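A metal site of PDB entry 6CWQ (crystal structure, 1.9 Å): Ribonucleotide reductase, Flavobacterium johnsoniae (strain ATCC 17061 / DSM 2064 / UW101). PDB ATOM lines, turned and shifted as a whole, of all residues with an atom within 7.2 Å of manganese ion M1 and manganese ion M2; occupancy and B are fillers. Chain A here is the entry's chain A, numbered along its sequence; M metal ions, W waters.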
ATOM      1  N   ILE A  68     -15.737  10.846   7.765  1.00  0.00           N
ATOM      2  CA  ILE A  68     -15.025  12.094   8.066  1.00  0.00           C
ATOM      3  C   ILE A  68     -14.306  12.058   9.427  1.00  0.00           C
ATOM      4  O   ILE A  68     -13.162  12.514   9.531  1.00  0.00           O
ATOM      5  CB  ILE A  68     -15.974  13.309   7.951  1.00  0.00           C
ATOM      6  CG1 ILE A  68     -16.278  13.579   6.472  1.00  0.00           C
ATOM      7  CG2 ILE A  68     -15.379  14.553   8.593  1.00  0.00           C
ATOM      8  CD1 ILE A  68     -17.416  14.529   6.235  1.00  0.00           C
ATOM      9  N   GLU A  69     -14.957  11.507  10.451  1.00  0.00           N
ATOM     10  CA  GLU A  69     -14.459  11.632  11.815  1.00  0.00           C
ATOM     11  C   GLU A  69     -13.409  10.597  12.219  1.00  0.00           C
ATOM     12  O   GLU A  69     -12.570  10.886  13.068  1.00  0.00           O
ATOM     13  CB  GLU A  69     -15.614  11.581  12.832  1.00  0.00           C
ATOM     14  CG  GLU A  69     -16.580  12.760  12.753  1.00  0.00           C
ATOM     15  CD  GLU A  69     -16.031  14.030  13.366  1.00  0.00           C
ATOM     16  OE1 GLU A  69     -14.814  14.185  13.504  1.00  0.00           O
ATOM     17  OE2 GLU A  69     -16.841  14.897  13.730  1.00  0.00           O
ATOM     18  N   LYS A  73      -6.847  13.847  11.223  1.00  0.00           N
ATOM     19  CA  LYS A  73      -7.248  15.161  10.711  1.00  0.00           C
ATOM     20  C   LYS A  73      -6.232  16.187  11.182  1.00  0.00           C
ATOM     21  O   LYS A  73      -6.257  16.589  12.342  1.00  0.00           O
ATOM     22  CB  LYS A  73      -8.661  15.513  11.204  1.00  0.00           C
ATOM     23  CG  LYS A  73      -9.781  14.640  10.664  1.00  0.00           C
ATOM     24  CD  LYS A  73     -11.005  14.604  11.575  1.00  0.00           C
ATOM     25  CE  LYS A  73     -10.832  13.618  12.730  1.00  0.00           C
ATOM     26  NZ  LYS A  73     -11.932  13.627  13.755  1.00  0.00           N
ATOM     27  N   TRP A  76      -6.322  21.609  11.669  1.00  0.00           N
ATOM     28  CA  TRP A  76      -6.312  22.546  12.806  1.00  0.00           C
ATOM     29  C   TRP A  76      -4.975  22.561  13.537  1.00  0.00           C
ATOM     30  O   TRP A  76      -4.460  23.632  13.868  1.00  0.00           O
ATOM     31  CB  TRP A  76      -7.442  22.229  13.781  1.00  0.00           C
ATOM     32  CG  TRP A  76      -8.769  22.667  13.276  1.00  0.00           C
ATOM     33  CD1 TRP A  76      -9.845  21.880  12.990  1.00  0.00           C
ATOM     34  CD2 TRP A  76      -9.164  24.011  12.978  1.00  0.00           C
ATOM     35  NE1 TRP A  76     -10.891  22.653  12.553  1.00  0.00           N
ATOM     36  CE2 TRP A  76     -10.496  23.966  12.518  1.00  0.00           C
ATOM     37  CE3 TRP A  76      -8.517  25.253  13.076  1.00  0.00           C
ATOM     38  CZ2 TRP A  76     -11.207  25.112  12.164  1.00  0.00           C
ATOM     39  CZ3 TRP A  76      -9.221  26.390  12.709  1.00  0.00           C
ATOM     40  CH2 TRP A  76     -10.552  26.314  12.254  1.00  0.00           C
ATOM     41  N   PHE A  95      -8.467  22.653  19.007  1.00  0.00           N
ATOM     42  CA  PHE A  95      -9.337  22.002  18.015  1.00  0.00           C
ATOM     43  C   PHE A  95      -8.777  20.651  17.552  1.00  0.00           C
ATOM     44  O   PHE A  95      -9.538  19.715  17.295  1.00  0.00           O
ATOM     45  CB  PHE A  95      -9.547  22.931  16.798  1.00  0.00           C
ATOM     46  CG  PHE A  95     -10.460  24.108  17.052  1.00  0.00           C
ATOM     47  CD1 PHE A  95     -10.968  24.399  18.316  1.00  0.00           C
ATOM     48  CD2 PHE A  95     -10.791  24.952  16.005  1.00  0.00           C
ATOM     49  CE1 PHE A  95     -11.800  25.484  18.517  1.00  0.00           C
ATOM     50  CE2 PHE A  95     -11.618  26.038  16.192  1.00  0.00           C
ATOM     51  CZ  PHE A  95     -12.137  26.305  17.443  1.00  0.00           C
ATOM     52  N   CYS A  98      -9.600  17.976  20.090  1.00  0.00           N
ATOM     53  CA  CYS A  98     -11.004  17.677  19.930  1.00  0.00           C
ATOM     54  C   CYS A  98     -11.244  16.574  18.881  1.00  0.00           C
ATOM     55  O   CYS A  98     -12.063  15.677  19.087  1.00  0.00           O
ATOM     56  CB  CYS A  98     -11.732  18.963  19.536  1.00  0.00           C
ATOM     57  SG  CYS A  98     -13.503  18.815  19.569  1.00  0.00           S
ATOM     58  N   GLU A  99     -10.525  16.671  17.763  1.00  0.00           N
ATOM     59  CA  GLU A  99     -10.703  15.713  16.671  1.00  0.00           C
ATOM     60  C   GLU A  99     -10.329  14.271  17.052  1.00  0.00           C
ATOM     61  O   GLU A  99     -10.869  13.320  16.488  1.00  0.00           O
ATOM     62  CB  GLU A  99      -9.949  16.174  15.428  1.00  0.00           C
ATOM     63  CG  GLU A  99     -10.577  17.387  14.726  1.00  0.00           C
ATOM     64  CD  GLU A  99     -12.074  17.233  14.470  1.00  0.00           C
ATOM     65  OE1 GLU A  99     -12.568  16.109  14.216  1.00  0.00           O
ATOM     66  OE2 GLU A  99     -12.789  18.267  14.527  1.00  0.00           O
ATOM     67  N   PHE A 100      -9.393  14.121  17.991  1.00  0.00           N
ATOM     68  CA  PHE A 100      -9.037  12.791  18.449  1.00  0.00           C
ATOM     69  C   PHE A 100     -10.116  12.257  19.395  1.00  0.00           C
ATOM     70  O   PHE A 100     -10.430  11.073  19.371  1.00  0.00           O
ATOM     71  CB  PHE A 100      -7.678  12.769  19.131  1.00  0.00           C
ATOM     72  CG  PHE A 100      -7.210  11.398  19.512  1.00  0.00           C
ATOM     73  CD1 PHE A 100      -7.000  10.443  18.523  1.00  0.00           C
ATOM     74  CD2 PHE A 100      -6.969  11.071  20.829  1.00  0.00           C
ATOM     75  CE1 PHE A 100      -6.573   9.173  18.860  1.00  0.00           C
ATOM     76  CE2 PHE A 100      -6.527   9.796  21.171  1.00  0.00           C
ATOM     77  CZ  PHE A 100      -6.328   8.847  20.186  1.00  0.00           C
ATOM     78  N   HIS A 102     -13.199  12.965  18.996  1.00  0.00           N
ATOM     79  CA  HIS A 102     -14.218  12.572  18.025  1.00  0.00           C
ATOM     80  C   HIS A 102     -13.928  11.252  17.321  1.00  0.00           C
ATOM     81  O   HIS A 102     -14.812  10.397  17.216  1.00  0.00           O
ATOM     82  CB  HIS A 102     -14.401  13.642  16.970  1.00  0.00           C
ATOM     83  CG  HIS A 102     -14.962  14.921  17.503  1.00  0.00           C
ATOM     84  ND1 HIS A 102     -15.151  16.029  16.711  1.00  0.00           N
ATOM     85  CD2 HIS A 102     -15.373  15.263  18.736  1.00  0.00           C
ATOM     86  CE1 HIS A 102     -15.652  17.009  17.437  1.00  0.00           C
ATOM     87  NE2 HIS A 102     -15.800  16.563  18.672  1.00  0.00           N
ATOM     88  N   SER A 103     -12.701  11.083  16.823  1.00  0.00           N
ATOM     89  CA  SER A 103     -12.344   9.848  16.119  1.00  0.00           C
ATOM     90  C   SER A 103     -12.510   8.640  17.043  1.00  0.00           C
ATOM     91  O   SER A 103     -13.011   7.591  16.613  1.00  0.00           O
ATOM     92  CB  SER A 103     -10.924   9.916  15.525  1.00  0.00           C
ATOM     93  OG  SER A 103      -9.910  10.034  16.504  1.00  0.00           O
ATOM     94  N   TYR A 106     -16.399   7.931  17.483  1.00  0.00           N
ATOM     95  CA  TYR A 106     -17.051   7.250  16.354  1.00  0.00           C
ATOM     96  C   TYR A 106     -16.487   5.877  16.070  1.00  0.00           C
ATOM     97  O   TYR A 106     -17.225   4.994  15.638  1.00  0.00           O
ATOM     98  CB  TYR A 106     -17.130   8.169  15.114  1.00  0.00           C
ATOM     99  CG  TYR A 106     -18.094   9.279  15.435  1.00  0.00           C
ATOM    100  CD1 TYR A 106     -19.473   9.055  15.395  1.00  0.00           C
ATOM    101  CD2 TYR A 106     -17.644  10.501  15.891  1.00  0.00           C
ATOM    102  CE1 TYR A 106     -20.372  10.050  15.752  1.00  0.00           C
ATOM    103  CE2 TYR A 106     -18.535  11.500  16.267  1.00  0.00           C
ATOM    104  CZ  TYR A 106     -19.894  11.271  16.195  1.00  0.00           C
ATOM    105  OH  TYR A 106     -20.757  12.257  16.572  1.00  0.00           O
ATOM    106  N   PHE A 157     -13.004  24.443   3.994  1.00  0.00           N
ATOM    107  CA  PHE A 157     -12.891  23.597   5.184  1.00  0.00           C
ATOM    108  C   PHE A 157     -13.945  23.989   6.231  1.00  0.00           C
ATOM    109  O   PHE A 157     -14.645  23.132   6.765  1.00  0.00           O
ATOM    110  CB  PHE A 157     -11.481  23.672   5.771  1.00  0.00           C
ATOM    111  CG  PHE A 157     -11.237  22.740   6.917  1.00  0.00           C
ATOM    112  CD1 PHE A 157     -10.797  21.444   6.687  1.00  0.00           C
ATOM    113  CD2 PHE A 157     -11.455  23.137   8.221  1.00  0.00           C
ATOM    114  CE1 PHE A 157     -10.577  20.565   7.746  1.00  0.00           C
ATOM    115  CE2 PHE A 157     -11.245  22.275   9.271  1.00  0.00           C
ATOM    116  CZ  PHE A 157     -10.808  20.988   9.039  1.00  0.00           C
ATOM    117  N   ILE A 161     -16.504  21.040   5.543  1.00  0.00           N
ATOM    118  CA  ILE A 161     -16.042  19.970   6.439  1.00  0.00           C
ATOM    119  C   ILE A 161     -16.571  20.145   7.867  1.00  0.00           C
ATOM    120  O   ILE A 161     -16.935  19.158   8.507  1.00  0.00           O
ATOM    121  CB  ILE A 161     -14.510  19.866   6.515  1.00  0.00           C
ATOM    122  CG1 ILE A 161     -13.862  19.741   5.124  1.00  0.00           C
ATOM    123  CG2 ILE A 161     -14.076  18.681   7.377  1.00  0.00           C
ATOM    124  CD1 ILE A 161     -14.357  18.576   4.312  1.00  0.00           C
ATOM    125  N   GLU A 162     -16.586  21.378   8.374  1.00  0.00           N
ATOM    126  CA  GLU A 162     -16.980  21.647   9.757  1.00  0.00           C
ATOM    127  C   GLU A 162     -18.466  21.975   9.954  1.00  0.00           C
ATOM    128  O   GLU A 162     -19.026  21.654  10.996  1.00  0.00           O
ATOM    129  CB  GLU A 162     -16.159  22.804  10.336  1.00  0.00           C
ATOM    130  CG  GLU A 162     -14.665  22.649  10.215  1.00  0.00           C
ATOM    131  CD  GLU A 162     -14.123  21.442  10.956  1.00  0.00           C
ATOM    132  OE1 GLU A 162     -13.414  21.631  11.948  1.00  0.00           O
ATOM    133  OE2 GLU A 162     -14.413  20.304  10.546  1.00  0.00           O
ATOM    134  N   LEU A 166     -21.321  17.039   7.780  1.00  0.00           N
ATOM    135  CA  LEU A 166     -21.739  16.112   8.833  1.00  0.00           C
ATOM    136  C   LEU A 166     -23.176  16.351   9.324  1.00  0.00           C
ATOM    137  O   LEU A 166     -23.805  15.432   9.849  1.00  0.00           O
ATOM    138  CB  LEU A 166     -20.812  16.242  10.038  1.00  0.00           C
ATOM    139  CG  LEU A 166     -19.346  15.855   9.838  1.00  0.00           C
ATOM    140  CD1 LEU A 166     -18.481  16.384  10.977  1.00  0.00           C
ATOM    141  CD2 LEU A 166     -19.216  14.349   9.740  1.00  0.00           C
ATOM    142  N   PHE A 170     -25.961  14.138  11.583  1.00  0.00           N
ATOM    143  CA  PHE A 170     -26.270  14.477  12.971  1.00  0.00           C
ATOM    144  C   PHE A 170     -27.786  14.607  13.172  1.00  0.00           C
ATOM    145  O   PHE A 170     -28.358  14.004  14.092  1.00  0.00           O
ATOM    146  CB  PHE A 170     -25.596  15.791  13.398  1.00  0.00           C
ATOM    147  CG  PHE A 170     -24.083  15.744  13.450  1.00  0.00           C
ATOM    148  CD1 PHE A 170     -23.382  14.554  13.571  1.00  0.00           C
ATOM    149  CD2 PHE A 170     -23.372  16.939  13.438  1.00  0.00           C
ATOM    150  CE1 PHE A 170     -22.008  14.558  13.654  1.00  0.00           C
ATOM    151  CE2 PHE A 170     -21.978  16.938  13.513  1.00  0.00           C
ATOM    152  CZ  PHE A 170     -21.305  15.749  13.625  1.00  0.00           C
ATOM    153  N   THR A 193     -20.755  16.259  19.728  1.00  0.00           N
ATOM    154  CA  THR A 193     -19.977  16.455  18.511  1.00  0.00           C
ATOM    155  C   THR A 193     -20.459  17.681  17.740  1.00  0.00           C
ATOM    156  O   THR A 193     -19.636  18.476  17.272  1.00  0.00           O
ATOM    157  CB  THR A 193     -20.037  15.226  17.581  1.00  0.00           C
ATOM    158  OG1 THR A 193     -19.643  14.054  18.304  1.00  0.00           O
ATOM    159  CG2 THR A 193     -19.101  15.411  16.395  1.00  0.00           C
ATOM    160  N   ASP A 196     -19.163  20.908  19.333  1.00  0.00           N
ATOM    161  CA  ASP A 196     -17.750  21.087  18.978  1.00  0.00           C
ATOM    162  C   ASP A 196     -17.581  21.552  17.541  1.00  0.00           C
ATOM    163  O   ASP A 196     -16.835  22.487  17.283  1.00  0.00           O
ATOM    164  CB  ASP A 196     -16.943  19.798  19.181  1.00  0.00           C
ATOM    165  CG  ASP A 196     -16.781  19.429  20.640  1.00  0.00           C
ATOM    166  OD1 ASP A 196     -16.954  20.288  21.530  1.00  0.00           O
ATOM    167  OD2 ASP A 196     -16.475  18.233  20.896  1.00  0.00           O
ATOM    168  N   GLU A 197     -18.272  20.897  16.603  1.00  0.00           N
ATOM    169  CA  GLU A 197     -18.089  21.211  15.198  1.00  0.00           C
ATOM    170  C   GLU A 197     -18.534  22.623  14.888  1.00  0.00           C
ATOM    171  O   GLU A 197     -17.915  23.308  14.065  1.00  0.00           O
ATOM    172  CB  GLU A 197     -18.859  20.248  14.284  1.00  0.00           C
ATOM    173  CG  GLU A 197     -18.393  18.812  14.322  1.00  0.00           C
ATOM    174  CD  GLU A 197     -16.913  18.637  14.045  1.00  0.00           C
ATOM    175  OE1 GLU A 197     -16.263  19.563  13.520  1.00  0.00           O
ATOM    176  OE2 GLU A 197     -16.404  17.550  14.356  1.00  0.00           O
ATOM    177  N   GLN A 198     -19.601  23.060  15.544  1.00  0.00           N
ATOM    178  CA  GLN A 198     -20.092  24.420  15.364  1.00  0.00           C
ATOM    179  C   GLN A 198     -19.072  25.447  15.821  1.00  0.00           C
ATOM    180  O   GLN A 198     -18.860  26.470  15.176  1.00  0.00           O
ATOM    181  CB  GLN A 198     -21.421  24.629  16.100  1.00  0.00           C
ATOM    182  CG  GLN A 198     -22.081  25.938  15.739  1.00  0.00           C
ATOM    183  CD  GLN A 198     -22.370  26.002  14.258  1.00  0.00           C
ATOM    184  OE1 GLN A 198     -23.127  25.195  13.743  1.00  0.00           O
ATOM    185  NE2 GLN A 198     -21.758  26.952  13.557  1.00  0.00           N
ATOM    186  N   HIS A 200     -15.854  24.864  15.849  1.00  0.00           N
ATOM    187  CA  HIS A 200     -14.797  24.810  14.829  1.00  0.00           C
ATOM    188  C   HIS A 200     -15.147  25.706  13.636  1.00  0.00           C
ATOM    189  O   HIS A 200     -14.318  26.482  13.192  1.00  0.00           O
ATOM    190  CB  HIS A 200     -14.504  23.384  14.343  1.00  0.00           C
ATOM    191  CG  HIS A 200     -14.051  22.465  15.427  1.00  0.00           C
ATOM    192  ND1 HIS A 200     -13.936  21.108  15.252  1.00  0.00           N
ATOM    193  CD2 HIS A 200     -13.715  22.703  16.721  1.00  0.00           C
ATOM    194  CE1 HIS A 200     -13.535  20.541  16.374  1.00  0.00           C
ATOM    195  NE2 HIS A 200     -13.399  21.490  17.286  1.00  0.00           N
ATOM    196  N   ALA A 201     -16.360  25.571  13.127  1.00  0.00           N
ATOM    197  CA  ALA A 201     -16.843  26.396  12.018  1.00  0.00           C
ATOM    198  C   ALA A 201     -16.776  27.880  12.355  1.00  0.00           C
ATOM    199  O   ALA A 201     -16.288  28.680  11.548  1.00  0.00           O
ATOM    200  CB  ALA A 201     -18.268  26.009  11.650  1.00  0.00           C
HETATM  201 MN    MN M   1     -14.982  16.286  14.412  1.00  0.00          MN
HETATM  202 MN    MN M   2     -14.163  19.686  13.389  1.00  0.00          MN
HETATM  203  O   HOH W   1     -14.836  17.490  11.787  1.00  0.00           O
HETATM  204  O   HOH W   2     -12.295  19.071  12.006  1.00  0.00           O
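The side-chain carboxylate (OE1) of Glu 197 is bound to manganese ion M2, 2.1 Å away. Manganese ion M2 is bound by the side-chain carboxylate (OE2) of Glu 99 (2.3 Å). ND1 of His 200 is bound to manganese ion M2, at 2.4 Å. Water W2 is bound to manganese ion M2 (2.4 Å). The side-chain carboxylate (OE1) of Glu 162 is bound to manganese ion M2 (2.5 Å). Manganese ion M2 has five donor atoms within binding distance. Slightly farther from manganese ion M2 lies water W1 (2.8 Å). Slightly farther from manganese ion M2 lies the side-chain carboxylate (OE2) of Glu 162 (2.9 Å).
Manganese ion M1 is bound by OE2 of Glu 197, 1.9 Å away. Manganese ion M1 is bound by the side-chain carboxylate (OE1) of Glu 69, at 2.3 Å. Manganese ion M1 is bound by ND1 of His 102. OE2 of Glu 69 binds manganese ion M1 (2.4 Å). OE1 of Glu 99 is bound to manganese ion M1, at 2.4 Å. Manganese ion M1 has five donor atoms within binding distance. Slightly farther from manganese ion M1 lies water W1 (2.9 Å).
Of the 22 residues printed, 4 come within 4 Å of manganese ion M2. The nearest printed residue that does not touch manganese ion M2 is Trp 76 (4.5 Å).
NE2 of His 102 lies within hydrogen-bond range of SG of Cys 98 (3.3 Å). O of Glu 99 sits at hydrogen-bond distance from OG of Ser 103, 3.4 Å away. A ring nitrogen (NE2) of His 200 lies within hydrogen-bond range of the side-chain sulfur of Cys 98 (3.5 Å). The side-chain amino group (NZ) of Lys 73 sits at hydrogen-bond distance from the backbone carbonyl oxygen (O) of Glu 99, 2.9 Å away. The backbone carbonyl oxygen (O) of Glu 69 lies within hydrogen-bond range of the side-chain amino group (NZ) of Lys 73 (2.9 Å). A ring nitrogen (NE2) of His 102 lies within hydrogen-bond range of the side-chain carboxylate of Asp 196 (2.9 Å). OE1 of Glu 162 sits close to NE1 of Trp 76, 2.8 Å away. The backbone carbonyl oxygen (O) of Phe 157 is in hydrogen-bond range of the backbone NH (N) of Glu 162 (3.1 Å).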
